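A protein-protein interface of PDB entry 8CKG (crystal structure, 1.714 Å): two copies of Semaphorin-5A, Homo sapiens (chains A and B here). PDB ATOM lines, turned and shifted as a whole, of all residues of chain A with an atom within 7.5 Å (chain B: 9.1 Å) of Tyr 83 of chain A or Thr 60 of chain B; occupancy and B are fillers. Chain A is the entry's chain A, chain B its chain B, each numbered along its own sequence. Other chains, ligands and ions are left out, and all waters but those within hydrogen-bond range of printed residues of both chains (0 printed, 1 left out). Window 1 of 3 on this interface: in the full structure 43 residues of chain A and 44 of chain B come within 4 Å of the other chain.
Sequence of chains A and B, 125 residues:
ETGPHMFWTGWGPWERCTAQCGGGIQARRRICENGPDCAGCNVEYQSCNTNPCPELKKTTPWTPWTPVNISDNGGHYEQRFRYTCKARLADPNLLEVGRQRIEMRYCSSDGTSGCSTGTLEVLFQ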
ATOM      1  N   LYS A  58      -7.610 -22.676  11.441  1.00  0.00           N
ATOM      2  CA  LYS A  58      -7.318 -21.264  11.233  1.00  0.00           C
ATOM      3  C   LYS A  58      -5.809 -21.114  11.182  1.00  0.00           C
ATOM      4  O   LYS A  58      -5.106 -21.671  12.028  1.00  0.00           O
ATOM      5  CB  LYS A  58      -7.919 -20.412  12.356  1.00  0.00           C
ATOM      6  CG  LYS A  58      -9.427 -20.229  12.199  1.00  0.00           C
ATOM      7  CD  LYS A  58     -10.038 -19.462  13.365  1.00  0.00           C
ATOM      8  CE  LYS A  58     -11.569 -19.310  13.239  1.00  0.00           C
ATOM      9  NZ  LYS A  58     -12.047 -18.280  14.218  1.00  0.00           N
ATOM     10  N   THR A  59      -5.314 -20.376  10.199  1.00  0.00           N
ATOM     11  CA  THR A  59      -3.887 -20.116  10.125  1.00  0.00           C
ATOM     12  C   THR A  59      -3.493 -19.010  11.104  1.00  0.00           C
ATOM     13  O   THR A  59      -4.246 -18.055  11.332  1.00  0.00           O
ATOM     14  CB  THR A  59      -3.492 -19.736   8.688  1.00  0.00           C
ATOM     15  OG1 THR A  59      -2.094 -19.427   8.658  1.00  0.00           O
ATOM     16  CG2 THR A  59      -4.232 -18.489   8.239  1.00  0.00           C
ATOM     17  N   THR A  60      -2.276 -19.119  11.656  1.00  0.00           N
ATOM     18  CA  THR A  60      -1.693 -17.993  12.375  1.00  0.00           C
ATOM     19  C   THR A  60      -1.234 -16.940  11.372  1.00  0.00           C
ATOM     20  O   THR A  60      -0.995 -17.240  10.194  1.00  0.00           O
ATOM     21  CB  THR A  60      -0.486 -18.417  13.250  1.00  0.00           C
ATOM     22  OG1 THR A  60       0.676 -18.620  12.423  1.00  0.00           O
ATOM     23  CG2 THR A  60      -0.757 -19.672  14.057  1.00  0.00           C
ATOM     24  N   PRO A  61      -1.099 -15.687  11.810  1.00  0.00           N
ATOM     25  CA  PRO A  61      -0.390 -14.703  10.992  1.00  0.00           C
ATOM     26  C   PRO A  61       1.012 -15.198  10.655  1.00  0.00           C
ATOM     27  O   PRO A  61       1.591 -16.026  11.367  1.00  0.00           O
ATOM     28  CB  PRO A  61      -0.344 -13.462  11.895  1.00  0.00           C
ATOM     29  CG  PRO A  61      -1.491 -13.640  12.829  1.00  0.00           C
ATOM     30  CD  PRO A  61      -1.584 -15.114  13.080  1.00  0.00           C
ATOM     31  N   TRP A  62       1.547 -14.695   9.546  1.00  0.00           N
ATOM     32  CA  TRP A  62       2.962 -14.873   9.252  1.00  0.00           C
ATOM     33  C   TRP A  62       3.818 -14.098  10.245  1.00  0.00           C
ATOM     34  O   TRP A  62       3.482 -12.977  10.648  1.00  0.00           O
ATOM     35  CB  TRP A  62       3.300 -14.371   7.849  1.00  0.00           C
ATOM     36  CG  TRP A  62       2.809 -15.204   6.698  1.00  0.00           C
ATOM     37  CD1 TRP A  62       1.817 -14.884   5.809  1.00  0.00           C
ATOM     38  CD2 TRP A  62       3.330 -16.469   6.287  1.00  0.00           C
ATOM     39  NE1 TRP A  62       1.680 -15.893   4.872  1.00  0.00           N
ATOM     40  CE2 TRP A  62       2.593 -16.881   5.150  1.00  0.00           C
ATOM     41  CE3 TRP A  62       4.334 -17.306   6.784  1.00  0.00           C
ATOM     42  CZ2 TRP A  62       2.833 -18.099   4.499  1.00  0.00           C
ATOM     43  CZ3 TRP A  62       4.569 -18.531   6.137  1.00  0.00           C
ATOM     44  CH2 TRP A  62       3.826 -18.903   4.999  1.00  0.00           C
ATOM     45  N   THR A  63       4.960 -14.678  10.609  1.00  0.00           N
ATOM     46  CA  THR A  63       5.986 -13.911  11.291  1.00  0.00           C
ATOM     47  C   THR A  63       6.494 -12.817  10.350  1.00  0.00           C
ATOM     48  O   THR A  63       6.175 -12.834   9.146  1.00  0.00           O
ATOM     49  CB  THR A  63       7.128 -14.830  11.728  1.00  0.00           C
ATOM     50  OG1 THR A  63       7.738 -15.386  10.561  1.00  0.00           O
ATOM     51  CG2 THR A  63       6.613 -15.957  12.600  1.00  0.00           C
ATOM     52  N   PHE A  81       7.390 -17.585   8.754  1.00  0.00           N
ATOM     53  CA  PHE A  81       6.833 -18.830   9.268  1.00  0.00           C
ATOM     54  C   PHE A  81       5.385 -18.623   9.669  1.00  0.00           C
ATOM     55  O   PHE A  81       4.975 -17.516  10.036  1.00  0.00           O
ATOM     56  CB  PHE A  81       7.611 -19.338  10.496  1.00  0.00           C
ATOM     57  CG  PHE A  81       9.101 -19.437  10.277  1.00  0.00           C
ATOM     58  CD1 PHE A  81       9.919 -18.336  10.509  1.00  0.00           C
ATOM     59  CD2 PHE A  81       9.673 -20.622   9.855  1.00  0.00           C
ATOM     60  CE1 PHE A  81      11.279 -18.400  10.311  1.00  0.00           C
ATOM     61  CE2 PHE A  81      11.050 -20.705   9.660  1.00  0.00           C
ATOM     62  CZ  PHE A  81      11.851 -19.586   9.882  1.00  0.00           C
ATOM     63  N   ARG A  82       4.606 -19.693   9.605  1.00  0.00           N
ATOM     64  CA  ARG A  82       3.276 -19.690  10.207  1.00  0.00           C
ATOM     65  C   ARG A  82       2.949 -21.105  10.650  1.00  0.00           C
ATOM     66  O   ARG A  82       3.652 -22.062  10.317  1.00  0.00           O
ATOM     67  CB  ARG A  82       2.206 -19.135   9.256  1.00  0.00           C
ATOM     68  CG  ARG A  82       1.860 -19.949   7.989  1.00  0.00           C
ATOM     69  CD  ARG A  82       0.808 -19.186   7.173  1.00  0.00           C
ATOM     70  NE  ARG A  82       0.189 -19.909   6.062  1.00  0.00           N
ATOM     71  CZ  ARG A  82      -0.747 -19.395   5.262  1.00  0.00           C
ATOM     72  NH1 ARG A  82      -1.215 -18.164   5.431  1.00  0.00           N
ATOM     73  NH2 ARG A  82      -1.223 -20.132   4.259  1.00  0.00           N
ATOM     74  N   TYR A  83       1.866 -21.224  11.406  1.00  0.00           N
ATOM     75  CA  TYR A  83       1.313 -22.506  11.818  1.00  0.00           C
ATOM     76  C   TYR A  83      -0.169 -22.489  11.517  1.00  0.00           C
ATOM     77  O   TYR A  83      -0.719 -21.477  11.079  1.00  0.00           O
ATOM     78  CB  TYR A  83       1.533 -22.765  13.312  1.00  0.00           C
ATOM     79  CG  TYR A  83       2.967 -22.905  13.708  1.00  0.00           C
ATOM     80  CD1 TYR A  83       3.708 -21.790  14.064  1.00  0.00           C
ATOM     81  CD2 TYR A  83       3.583 -24.156  13.747  1.00  0.00           C
ATOM     82  CE1 TYR A  83       5.043 -21.912  14.436  1.00  0.00           C
ATOM     83  CE2 TYR A  83       4.911 -24.281  14.112  1.00  0.00           C
ATOM     84  CZ  TYR A  83       5.625 -23.161  14.468  1.00  0.00           C
ATOM     85  OH  TYR A  83       6.949 -23.277  14.832  1.00  0.00           O
ATOM     86  N   THR A  84      -0.819 -23.615  11.748  1.00  0.00           N
ATOM     87  CA  THR A  84      -2.265 -23.729  11.685  1.00  0.00           C
ATOM     88  C   THR A  84      -2.754 -24.136  13.074  1.00  0.00           C
ATOM     89  O   THR A  84      -2.078 -24.896  13.773  1.00  0.00           O
ATOM     90  CB  THR A  84      -2.686 -24.749  10.627  1.00  0.00           C
ATOM     91  OG1 THR A  84      -2.142 -24.376   9.347  1.00  0.00           O
ATOM     92  CG2 THR A  84      -4.196 -24.820  10.506  1.00  0.00           C
ATOM     93  N   CYS A  85      -3.888 -23.579  13.503  1.00  0.00           N
ATOM     94  CA  CYS A  85      -4.563 -24.001  14.727  1.00  0.00           C
ATOM     95  C   CYS A  85      -5.774 -24.835  14.333  1.00  0.00           C
ATOM     96  O   CYS A  85      -6.550 -24.412  13.474  1.00  0.00           O
ATOM     97  CB  CYS A  85      -5.004 -22.785  15.544  1.00  0.00           C
ATOM     98  SG  CYS A  85      -3.639 -21.790  16.191  1.00  0.00           S
ATOM     99  N   VAL A  97      -6.826 -17.731  17.264  1.00  0.00           N
ATOM    100  CA  VAL A  97      -5.370 -17.664  17.297  1.00  0.00           C
ATOM    101  C   VAL A  97      -4.950 -16.544  18.238  1.00  0.00           C
ATOM    102  O   VAL A  97      -5.402 -15.401  18.102  1.00  0.00           O
ATOM    103  CB  VAL A  97      -4.791 -17.442  15.890  1.00  0.00           C
ATOM    104  CG1 VAL A  97      -3.267 -17.340  15.982  1.00  0.00           C
ATOM    105  CG2 VAL A  97      -5.207 -18.558  14.971  1.00  0.00           C
ATOM    106  N   LYS B  57      -5.855 -24.140  25.754  1.00  0.00           N
ATOM    107  CA  LYS B  57      -4.778 -23.514  24.994  1.00  0.00           C
ATOM    108  C   LYS B  57      -3.640 -24.491  24.754  1.00  0.00           C
ATOM    109  O   LYS B  57      -3.323 -25.333  25.602  1.00  0.00           O
ATOM    110  CB  LYS B  57      -4.205 -22.292  25.723  1.00  0.00           C
ATOM    111  CG  LYS B  57      -5.151 -21.125  25.870  1.00  0.00           C
ATOM    112  CD  LYS B  57      -4.414 -19.939  26.494  1.00  0.00           C
ATOM    113  CE  LYS B  57      -5.354 -18.790  26.826  1.00  0.00           C
ATOM    114  NZ  LYS B  57      -4.592 -17.602  27.304  1.00  0.00           N
ATOM    115  N   LYS B  58      -3.010 -24.347  23.593  1.00  0.00           N
ATOM    116  CA  LYS B  58      -1.743 -24.994  23.295  1.00  0.00           C
ATOM    117  C   LYS B  58      -0.879 -23.994  22.539  1.00  0.00           C
ATOM    118  O   LYS B  58      -1.380 -23.279  21.670  1.00  0.00           O
ATOM    119  CB  LYS B  58      -1.952 -26.273  22.463  1.00  0.00           C
ATOM    120  CG  LYS B  58      -2.528 -27.412  23.298  1.00  0.00           C
ATOM    121  CD  LYS B  58      -3.036 -28.526  22.432  1.00  0.00           C
ATOM    122  CE  LYS B  58      -3.375 -29.738  23.266  1.00  0.00           C
ATOM    123  NZ  LYS B  58      -3.587 -30.910  22.373  1.00  0.00           N
ATOM    124  N   THR B  59       0.403 -23.920  22.880  1.00  0.00           N
ATOM    125  CA  THR B  59       1.304 -23.041  22.145  1.00  0.00           C
ATOM    126  C   THR B  59       1.929 -23.783  20.965  1.00  0.00           C
ATOM    127  O   THR B  59       2.174 -24.995  21.007  1.00  0.00           O
ATOM    128  CB  THR B  59       2.405 -22.482  23.048  1.00  0.00           C
ATOM    129  OG1 THR B  59       3.317 -23.531  23.369  1.00  0.00           O
ATOM    130  CG2 THR B  59       1.827 -21.922  24.360  1.00  0.00           C
ATOM    131  N   THR B  60       2.164 -23.050  19.897  1.00  0.00           N
ATOM    132  CA  THR B  60       2.916 -23.604  18.800  1.00  0.00           C
ATOM    133  C   THR B  60       4.346 -23.822  19.284  1.00  0.00           C
ATOM    134  O   THR B  60       4.768 -23.248  20.291  1.00  0.00           O
ATOM    135  CB  THR B  60       2.919 -22.667  17.578  1.00  0.00           C
ATOM    136  OG1 THR B  60       3.700 -21.489  17.870  1.00  0.00           O
ATOM    137  CG2 THR B  60       1.492 -22.256  17.147  1.00  0.00           C
ATOM    138  N   PRO B  61       5.115 -24.653  18.586  1.00  0.00           N
ATOM    139  CA  PRO B  61       6.565 -24.647  18.806  1.00  0.00           C
ATOM    140  C   PRO B  61       7.142 -23.288  18.427  1.00  0.00           C
ATOM    141  O   PRO B  61       6.567 -22.540  17.626  1.00  0.00           O
ATOM    142  CB  PRO B  61       7.080 -25.738  17.859  1.00  0.00           C
ATOM    143  CG  PRO B  61       5.876 -26.542  17.497  1.00  0.00           C
ATOM    144  CD  PRO B  61       4.712 -25.619  17.552  1.00  0.00           C
ATOM    145  N   TRP B  62       8.291 -22.972  19.017  1.00  0.00           N
ATOM    146  CA  TRP B  62       9.058 -21.813  18.569  1.00  0.00           C
ATOM    147  C   TRP B  62       9.554 -22.015  17.144  1.00  0.00           C
ATOM    148  O   TRP B  62       9.957 -23.119  16.765  1.00  0.00           O
ATOM    149  CB  TRP B  62      10.269 -21.595  19.486  1.00  0.00           C
ATOM    150  CG  TRP B  62       9.954 -21.129  20.861  1.00  0.00           C
ATOM    151  CD1 TRP B  62      10.037 -21.844  22.001  1.00  0.00           C
ATOM    152  CD2 TRP B  62       9.522 -19.819  21.223  1.00  0.00           C
ATOM    153  NE1 TRP B  62       9.691 -21.056  23.072  1.00  0.00           N
ATOM    154  CE2 TRP B  62       9.343 -19.813  22.604  1.00  0.00           C
ATOM    155  CE3 TRP B  62       9.241 -18.653  20.492  1.00  0.00           C
ATOM    156  CZ2 TRP B  62       8.933 -18.672  23.305  1.00  0.00           C
ATOM    157  CZ3 TRP B  62       8.820 -17.525  21.184  1.00  0.00           C
ATOM    158  CH2 TRP B  62       8.658 -17.550  22.567  1.00  0.00           C
ATOM    159  N   THR B  63       9.537 -20.943  16.348  1.00  0.00           N
ATOM    160  CA  THR B  63      10.269 -20.939  15.085  1.00  0.00           C
ATOM    161  C   THR B  63      11.763 -21.016  15.407  1.00  0.00           C
ATOM    162  O   THR B  63      12.159 -20.838  16.557  1.00  0.00           O
ATOM    163  CB  THR B  63       9.950 -19.682  14.275  1.00  0.00           C
ATOM    164  OG1 THR B  63      10.467 -18.541  14.967  1.00  0.00           O
ATOM    165  CG2 THR B  63       8.445 -19.525  14.105  1.00  0.00           C
ATOM    166  N   PRO B  64      12.619 -21.282  14.418  1.00  0.00           N
ATOM    167  CA  PRO B  64      14.068 -21.194  14.655  1.00  0.00           C
ATOM    168  C   PRO B  64      14.519 -19.771  14.984  1.00  0.00           C
ATOM    169  O   PRO B  64      13.865 -18.782  14.654  1.00  0.00           O
ATOM    170  CB  PRO B  64      14.682 -21.682  13.336  1.00  0.00           C
ATOM    171  CG  PRO B  64      13.586 -21.630  12.337  1.00  0.00           C
ATOM    172  CD  PRO B  64      12.317 -21.859  13.093  1.00  0.00           C
ATOM    173  N   ARG B  80      12.985 -15.403  17.974  1.00  0.00           N
ATOM    174  CA  ARG B  80      12.114 -16.435  17.416  1.00  0.00           C
ATOM    175  C   ARG B  80      10.675 -16.113  17.802  1.00  0.00           C
ATOM    176  O   ARG B  80      10.417 -15.256  18.649  1.00  0.00           O
ATOM    177  CB  ARG B  80      12.514 -17.838  17.898  1.00  0.00           C
ATOM    178  CG  ARG B  80      12.652 -17.957  19.399  1.00  0.00           C
ATOM    179  CD  ARG B  80      13.121 -19.332  19.814  1.00  0.00           C
ATOM    180  NE  ARG B  80      13.119 -19.506  21.267  1.00  0.00           N
ATOM    181  CZ  ARG B  80      13.357 -20.659  21.877  1.00  0.00           C
ATOM    182  NH1 ARG B  80      13.664 -21.747  21.190  1.00  0.00           N
ATOM    183  NH2 ARG B  80      13.263 -20.725  23.203  1.00  0.00           N
ATOM    184  N   PHE B  81       9.729 -16.833  17.208  1.00  0.00           N
ATOM    185  CA  PHE B  81       8.310 -16.517  17.336  1.00  0.00           C
ATOM    186  C   PHE B  81       7.498 -17.763  17.699  1.00  0.00           C
ATOM    187  O   PHE B  81       7.909 -18.902  17.441  1.00  0.00           O
ATOM    188  CB  PHE B  81       7.783 -15.926  16.041  1.00  0.00           C
ATOM    189  CG  PHE B  81       8.568 -14.759  15.540  1.00  0.00           C
ATOM    190  CD1 PHE B  81       9.663 -14.942  14.701  1.00  0.00           C
ATOM    191  CD2 PHE B  81       8.223 -13.471  15.898  1.00  0.00           C
ATOM    192  CE1 PHE B  81      10.402 -13.844  14.238  1.00  0.00           C
ATOM    193  CE2 PHE B  81       8.957 -12.376  15.440  1.00  0.00           C
ATOM    194  CZ  PHE B  81      10.046 -12.561  14.615  1.00  0.00           C
ATOM    195  N   ARG B  82       6.329 -17.530  18.303  1.00  0.00           N
ATOM    196  CA  ARG B  82       5.320 -18.576  18.488  1.00  0.00           C
ATOM    197  C   ARG B  82       3.948 -17.925  18.647  1.00  0.00           C
ATOM    198  O   ARG B  82       3.822 -16.696  18.761  1.00  0.00           O
ATOM    199  CB  ARG B  82       5.625 -19.477  19.690  1.00  0.00           C
ATOM    200  CG  ARG B  82       5.448 -18.786  21.050  1.00  0.00           C
ATOM    201  CD  ARG B  82       5.708 -19.722  22.191  1.00  0.00           C
ATOM    202  NE  ARG B  82       5.802 -19.016  23.473  1.00  0.00           N
ATOM    203  CZ  ARG B  82       5.975 -19.606  24.648  1.00  0.00           C
ATOM    204  NH1 ARG B  82       6.103 -20.920  24.742  1.00  0.00           N
ATOM    205  NH2 ARG B  82       6.023 -18.860  25.758  1.00  0.00           N
ATOM    206  N   TYR B  83       2.916 -18.771  18.653  1.00  0.00           N
ATOM    207  CA  TYR B  83       1.548 -18.331  18.904  1.00  0.00           C
ATOM    208  C   TYR B  83       0.878 -19.318  19.844  1.00  0.00           C
ATOM    209  O   TYR B  83       1.383 -20.416  20.102  1.00  0.00           O
ATOM    210  CB  TYR B  83       0.718 -18.232  17.615  1.00  0.00           C
ATOM    211  CG  TYR B  83       1.255 -17.303  16.579  1.00  0.00           C
ATOM    212  CD1 TYR B  83       2.249 -17.714  15.697  1.00  0.00           C
ATOM    213  CD2 TYR B  83       0.744 -16.017  16.441  1.00  0.00           C
ATOM    214  CE1 TYR B  83       2.720 -16.877  14.732  1.00  0.00           C
ATOM    215  CE2 TYR B  83       1.212 -15.168  15.487  1.00  0.00           C
ATOM    216  CZ  TYR B  83       2.205 -15.591  14.627  1.00  0.00           C
ATOM    217  OH  TYR B  83       2.670 -14.723  13.665  1.00  0.00           O
ATOM    218  N   THR B  84      -0.277 -18.921  20.365  1.00  0.00           N
ATOM    219  CA  THR B  84      -1.125 -19.838  21.110  1.00  0.00           C
ATOM    220  C   THR B  84      -2.361 -20.145  20.277  1.00  0.00           C
ATOM    221  O   THR B  84      -2.892 -19.267  19.592  1.00  0.00           O
ATOM    222  CB  THR B  84      -1.534 -19.261  22.463  1.00  0.00           C
ATOM    223  OG1 THR B  84      -0.373 -18.745  23.127  1.00  0.00           O
ATOM    224  CG2 THR B  84      -2.134 -20.366  23.332  1.00  0.00           C
ATOM    225  N   CYS B  85      -2.761 -21.413  20.274  1.00  0.00           N
ATOM    226  CA  CYS B  85      -4.029 -21.838  19.699  1.00  0.00           C
ATOM    227  C   CYS B  85      -5.017 -22.030  20.840  1.00  0.00           C
ATOM    228  O   CYS B  85      -4.711 -22.719  21.819  1.00  0.00           O
ATOM    229  CB  CYS B  85      -3.866 -23.143  18.919  1.00  0.00           C
ATOM    230  SG  CYS B  85      -2.757 -23.083  17.484  1.00  0.00           S
ATOM    231  N   LYS B  86      -6.187 -21.408  20.727  1.00  0.00           N
ATOM    232  CA  LYS B  86      -7.174 -21.416  21.793  1.00  0.00           C
ATOM    233  C   LYS B  86      -8.513 -21.905  21.263  1.00  0.00           C
ATOM    234  O   LYS B  86      -8.956 -21.496  20.183  1.00  0.00           O
ATOM    235  CB  LYS B  86      -7.340 -20.021  22.393  1.00  0.00           C
ATOM    236  CG  LYS B  86      -6.019 -19.328  22.678  1.00  0.00           C
ATOM    237  CD  LYS B  86      -6.232 -17.942  23.279  1.00  0.00           C
ATOM    238  CE  LYS B  86      -6.845 -16.999  22.262  1.00  0.00           C
ATOM    239  NZ  LYS B  86      -6.781 -15.577  22.718  1.00  0.00           N
ATOM    240  N   GLU B  96      -5.261 -29.020  18.464  1.00  0.00           N
ATOM    241  CA  GLU B  96      -3.985 -29.453  17.910  1.00  0.00           C
ATOM    242  C   GLU B  96      -3.343 -28.314  17.128  1.00  0.00           C
ATOM    243  O   GLU B  96      -4.028 -27.535  16.460  1.00  0.00           O
ATOM    244  CB  GLU B  96      -4.168 -30.668  16.980  1.00  0.00           C
ATOM    245  CG  GLU B  96      -2.862 -31.436  16.749  1.00  0.00           C
ATOM    246  CD  GLU B  96      -2.984 -32.563  15.725  1.00  0.00           C
ATOM    247  OE1 GLU B  96      -3.829 -32.462  14.807  1.00  0.00           O
ATOM    248  OE2 GLU B  96      -2.219 -33.549  15.837  1.00  0.00           O
ATOM    249  N   VAL B  97      -2.015 -28.253  17.178  1.00  0.00           N
ATOM    250  CA  VAL B  97      -1.232 -27.327  16.367  1.00  0.00           C
ATOM    251  C   VAL B  97      -0.787 -28.058  15.110  1.00  0.00           C
ATOM    252  O   VAL B  97      -0.258 -29.176  15.186  1.00  0.00           O
ATOM    253  CB  VAL B  97      -0.016 -26.789  17.136  1.00  0.00           C
ATOM    254  CG1 VAL B  97       0.817 -25.906  16.198  1.00  0.00           C
ATOM    255  CG2 VAL B  97      -0.439 -26.024  18.407  1.00  0.00           C
ATOM    256  N   GLY B  98      -1.011 -27.445  13.952  1.00  0.00           N
ATOM    257  CA  GLY B  98      -0.612 -28.037  12.697  1.00  0.00           C
ATOM    258  C   GLY B  98       0.859 -27.810  12.440  1.00  0.00           C
ATOM    259  O   GLY B  98       1.607 -27.310  13.282  1.00  0.00           O
ATOM    260  N   ARG B  99       1.267 -28.191  11.235  1.00  0.00           N
ATOM    261  CA  ARG B  99       2.658 -28.124  10.818  1.00  0.00           C
ATOM    262  C   ARG B  99       3.138 -26.693  10.718  1.00  0.00           C
ATOM    263  O   ARG B  99       2.358 -25.764  10.496  1.00  0.00           O
ATOM    264  CB  ARG B  99       2.833 -28.779   9.459  1.00  0.00           C
ATOM    265  CG  ARG B  99       2.624 -30.257   9.507  1.00  0.00           C
ATOM    266  CD  ARG B  99       2.819 -30.872   8.143  1.00  0.00           C
ATOM    267  NE  ARG B  99       2.626 -32.311   8.225  1.00  0.00           N
ATOM    268  CZ  ARG B  99       1.467 -32.925   8.023  1.00  0.00           C
ATOM    269  NH1 ARG B  99       0.361 -32.248   7.736  1.00  0.00           N
ATOM    270  NH2 ARG B  99       1.415 -34.252   8.103  1.00  0.00           N
ATOM    271  N   GLN B 100       4.445 -26.526  10.862  1.00  0.00           N
ATOM    272  CA  GLN B 100       5.076 -25.251  10.560  1.00  0.00           C
ATOM    273  C   GLN B 100       5.162 -25.083   9.050  1.00  0.00           C
ATOM    274  O   GLN B 100       5.568 -26.006   8.338  1.00  0.00           O
ATOM    275  CB  GLN B 100       6.464 -25.199  11.178  1.00  0.00           C
ATOM    276  CG  GLN B 100       7.255 -23.919  10.898  1.00  0.00           C
ATOM    277  CD  GLN B 100       8.692 -24.101  11.348  1.00  0.00           C
ATOM    278  OE1 GLN B 100       9.556 -24.483  10.556  1.00  0.00           O
ATOM    279  NE2 GLN B 100       8.947 -23.876  12.641  1.00  0.00           N
ATOM    280  N   ARG B 101       4.761 -23.917   8.560  1.00  0.00           N
ATOM    281  CA  ARG B 101       4.825 -23.598   7.138  1.00  0.00           C
ATOM    282  C   ARG B 101       5.835 -22.483   6.931  1.00  0.00           C
ATOM    283  O   ARG B 101       5.831 -21.500   7.672  1.00  0.00           O
ATOM    284  CB  ARG B 101       3.467 -23.140   6.604  1.00  0.00           C
ATOM    285  CG  ARG B 101       2.346 -24.127   6.826  1.00  0.00           C
ATOM    286  CD  ARG B 101       2.179 -25.012   5.634  1.00  0.00           C
ATOM    287  NE  ARG B 101       1.305 -26.133   5.938  1.00  0.00           N
ATOM    288  CZ  ARG B 101       1.112 -27.159   5.127  1.00  0.00           C
ATOM    289  NH1 ARG B 101       1.686 -27.210   3.931  1.00  0.00           N
ATOM    290  NH2 ARG B 101       0.339 -28.165   5.532  1.00  0.00           N
ATOM    291  N   ILE B 102       6.696 -22.625   5.924  1.00  0.00           N
ATOM    292  CA  ILE B 102       7.769 -21.671   5.670  1.00  0.00           C
ATOM    293  C   ILE B 102       7.581 -21.088   4.281  1.00  0.00           C
ATOM    294  O   ILE B 102       7.425 -21.835   3.306  1.00  0.00           O
ATOM    295  CB  ILE B 102       9.154 -22.333   5.781  1.00  0.00           C
ATOM    296  CG1 ILE B 102       9.307 -23.033   7.139  1.00  0.00           C
ATOM    297  CG2 ILE B 102      10.277 -21.314   5.536  1.00  0.00           C
ATOM    298  CD1 ILE B 102      10.647 -23.691   7.326  1.00  0.00           C
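CZ3 of Trp 62 of chain A touches O of Arg 101 of chain B, 3.6 Å away. Phe 81 of chain A touches Pro 64 of chain B (CZ to CG, 3.6 Å). Phe 81 of chain A touches Gln 100 of chain B (CD2 to CD, 3.9 Å). Arg 101 of chain B touches Phe 81 of chain A (O to CA, 3.3 Å). O of Arg 82 of chain A touches CA of Gln 100 of chain B (3.5 Å). Tyr 83 of chain A touches Trp 62 of chain B (OH to O, 3.6 Å). Tyr 83 of chain A touches Thr 63 of chain B (OH to N, 3.8 Å). Gly 98 of chain B touches Tyr 83 of chain A. Val 97 of chain A touches Thr 84 of chain B.
The backbone carbonyl oxygen (O) of Lys 58 of chain A is in hydrogen-bond range of the backbone NH (N) of Cys 85 of chain A (2.7 Å). OG1 of Thr 59 of chain A sits at hydrogen-bond distance from O of Tyr 83 of chain A, 3.5 Å away. The backbone NH (N) of Thr 60 of chain B lies within hydrogen-bond range of the backbone carbonyl oxygen (O) of Tyr 83 of chain B (2.8 Å). N of Thr 63 of chain B lies within hydrogen-bond range of O of Phe 81 of chain B. OG1 of Thr 63 of chain A lies within hydrogen-bond range of N of Phe 81 of chain A, at 2.9 Å.
The backbone carbonyl oxygen (O) of Pro 61 of chain B is in hydrogen-bond range of the side-chain hydroxyl (OH) of Tyr 83 of chain A, at 2.9 Å. OH of Tyr 83 of chain A lies within hydrogen-bond range of NE2 of Gln 100 of chain B, at 3.0 Å. O of Thr 84 of chain A lies within hydrogen-bond range of N of Gly 98 of chain B (2.8 Å). The backbone carbonyl oxygen of Pro 61 of chain A sits at hydrogen-bond distance from the side-chain hydroxyl of Tyr 83 of chain B, at 2.9 Å. SG of Cys 85 of chain A forms a disulfide with SG of Cys 85 of chain B (2.0 Å). The backbone NH (N) of Arg 101 of chain B sits at hydrogen-bond distance from the backbone carbonyl oxygen (O) of Arg 82 of chain A.
Thr 60 of chain B touches just one residue of chain A: Tyr 83 (3.7 Å). Of chain B, only Val 97 and Gly 98 come within 4 Å of Thr 84 of chain A. Printed residues of chain A within 4 Å of Pro 64 of chain B: Phe 81. Of the printed residues of chain B, Arg 82 of chain A touches Arg 99, Gln 100 and Arg 101. Printed residues of chain A within 4 Å of Tyr 83 of chain B: Thr 60, Pro 61, Trp 62 and Thr 63. Of the printed residues of chain A, Arg 99 of chain B touches Arg 82 (3.9 Å) and Tyr 83 (3.7 Å). Lys 58 of chain B touches none of the printed residues of chain A. Thr 59 of chain A touches none of the printed residues of chain B. The nearest residue of chain A that does not touch Thr 60 of chain B is Thr 60 of chain A (4.6 Å). The nearest printed residue of chain A that does not touch Trp 62 of chain B is Phe 81 of chain A (7.3 Å).
Printed residues of chain B that touch a printed residue of chain A: Thr 60, Pro 61, Trp 62, Thr 63, Pro 64, Phe 81, Tyr 83, Thr 84, Cys 85, Glu 96, Val 97, Gly 98, Arg 99, Gln 100, Arg 101 and Ile 102. Along chain A the printed residues that touch a printed residue of chain B span positions 60 to 97. Among the printed residues, 26 pairs touch across the chains. Among the printed residues, no Asp or Glu carboxylate lies within 4 Å of a Lys or Arg side-chain nitrogen of the other chain.
Thr 63 of chain A touches Tyr 83 of chain B, and with the chains exchanged Tyr 83 of chain A touches Thr 63 of chain B. Thr 84 of chain A touches Val 97 of chain B, and with the chains exchanged Val 97 of chain A touches Thr 84 of chain B. Cys 85 of chain A touches its own counterpart, Cys 85 of chain B. Of the 26 pairs that touch across the chains among the printed residues, 13 have their exchanged pair printed and touching as well.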
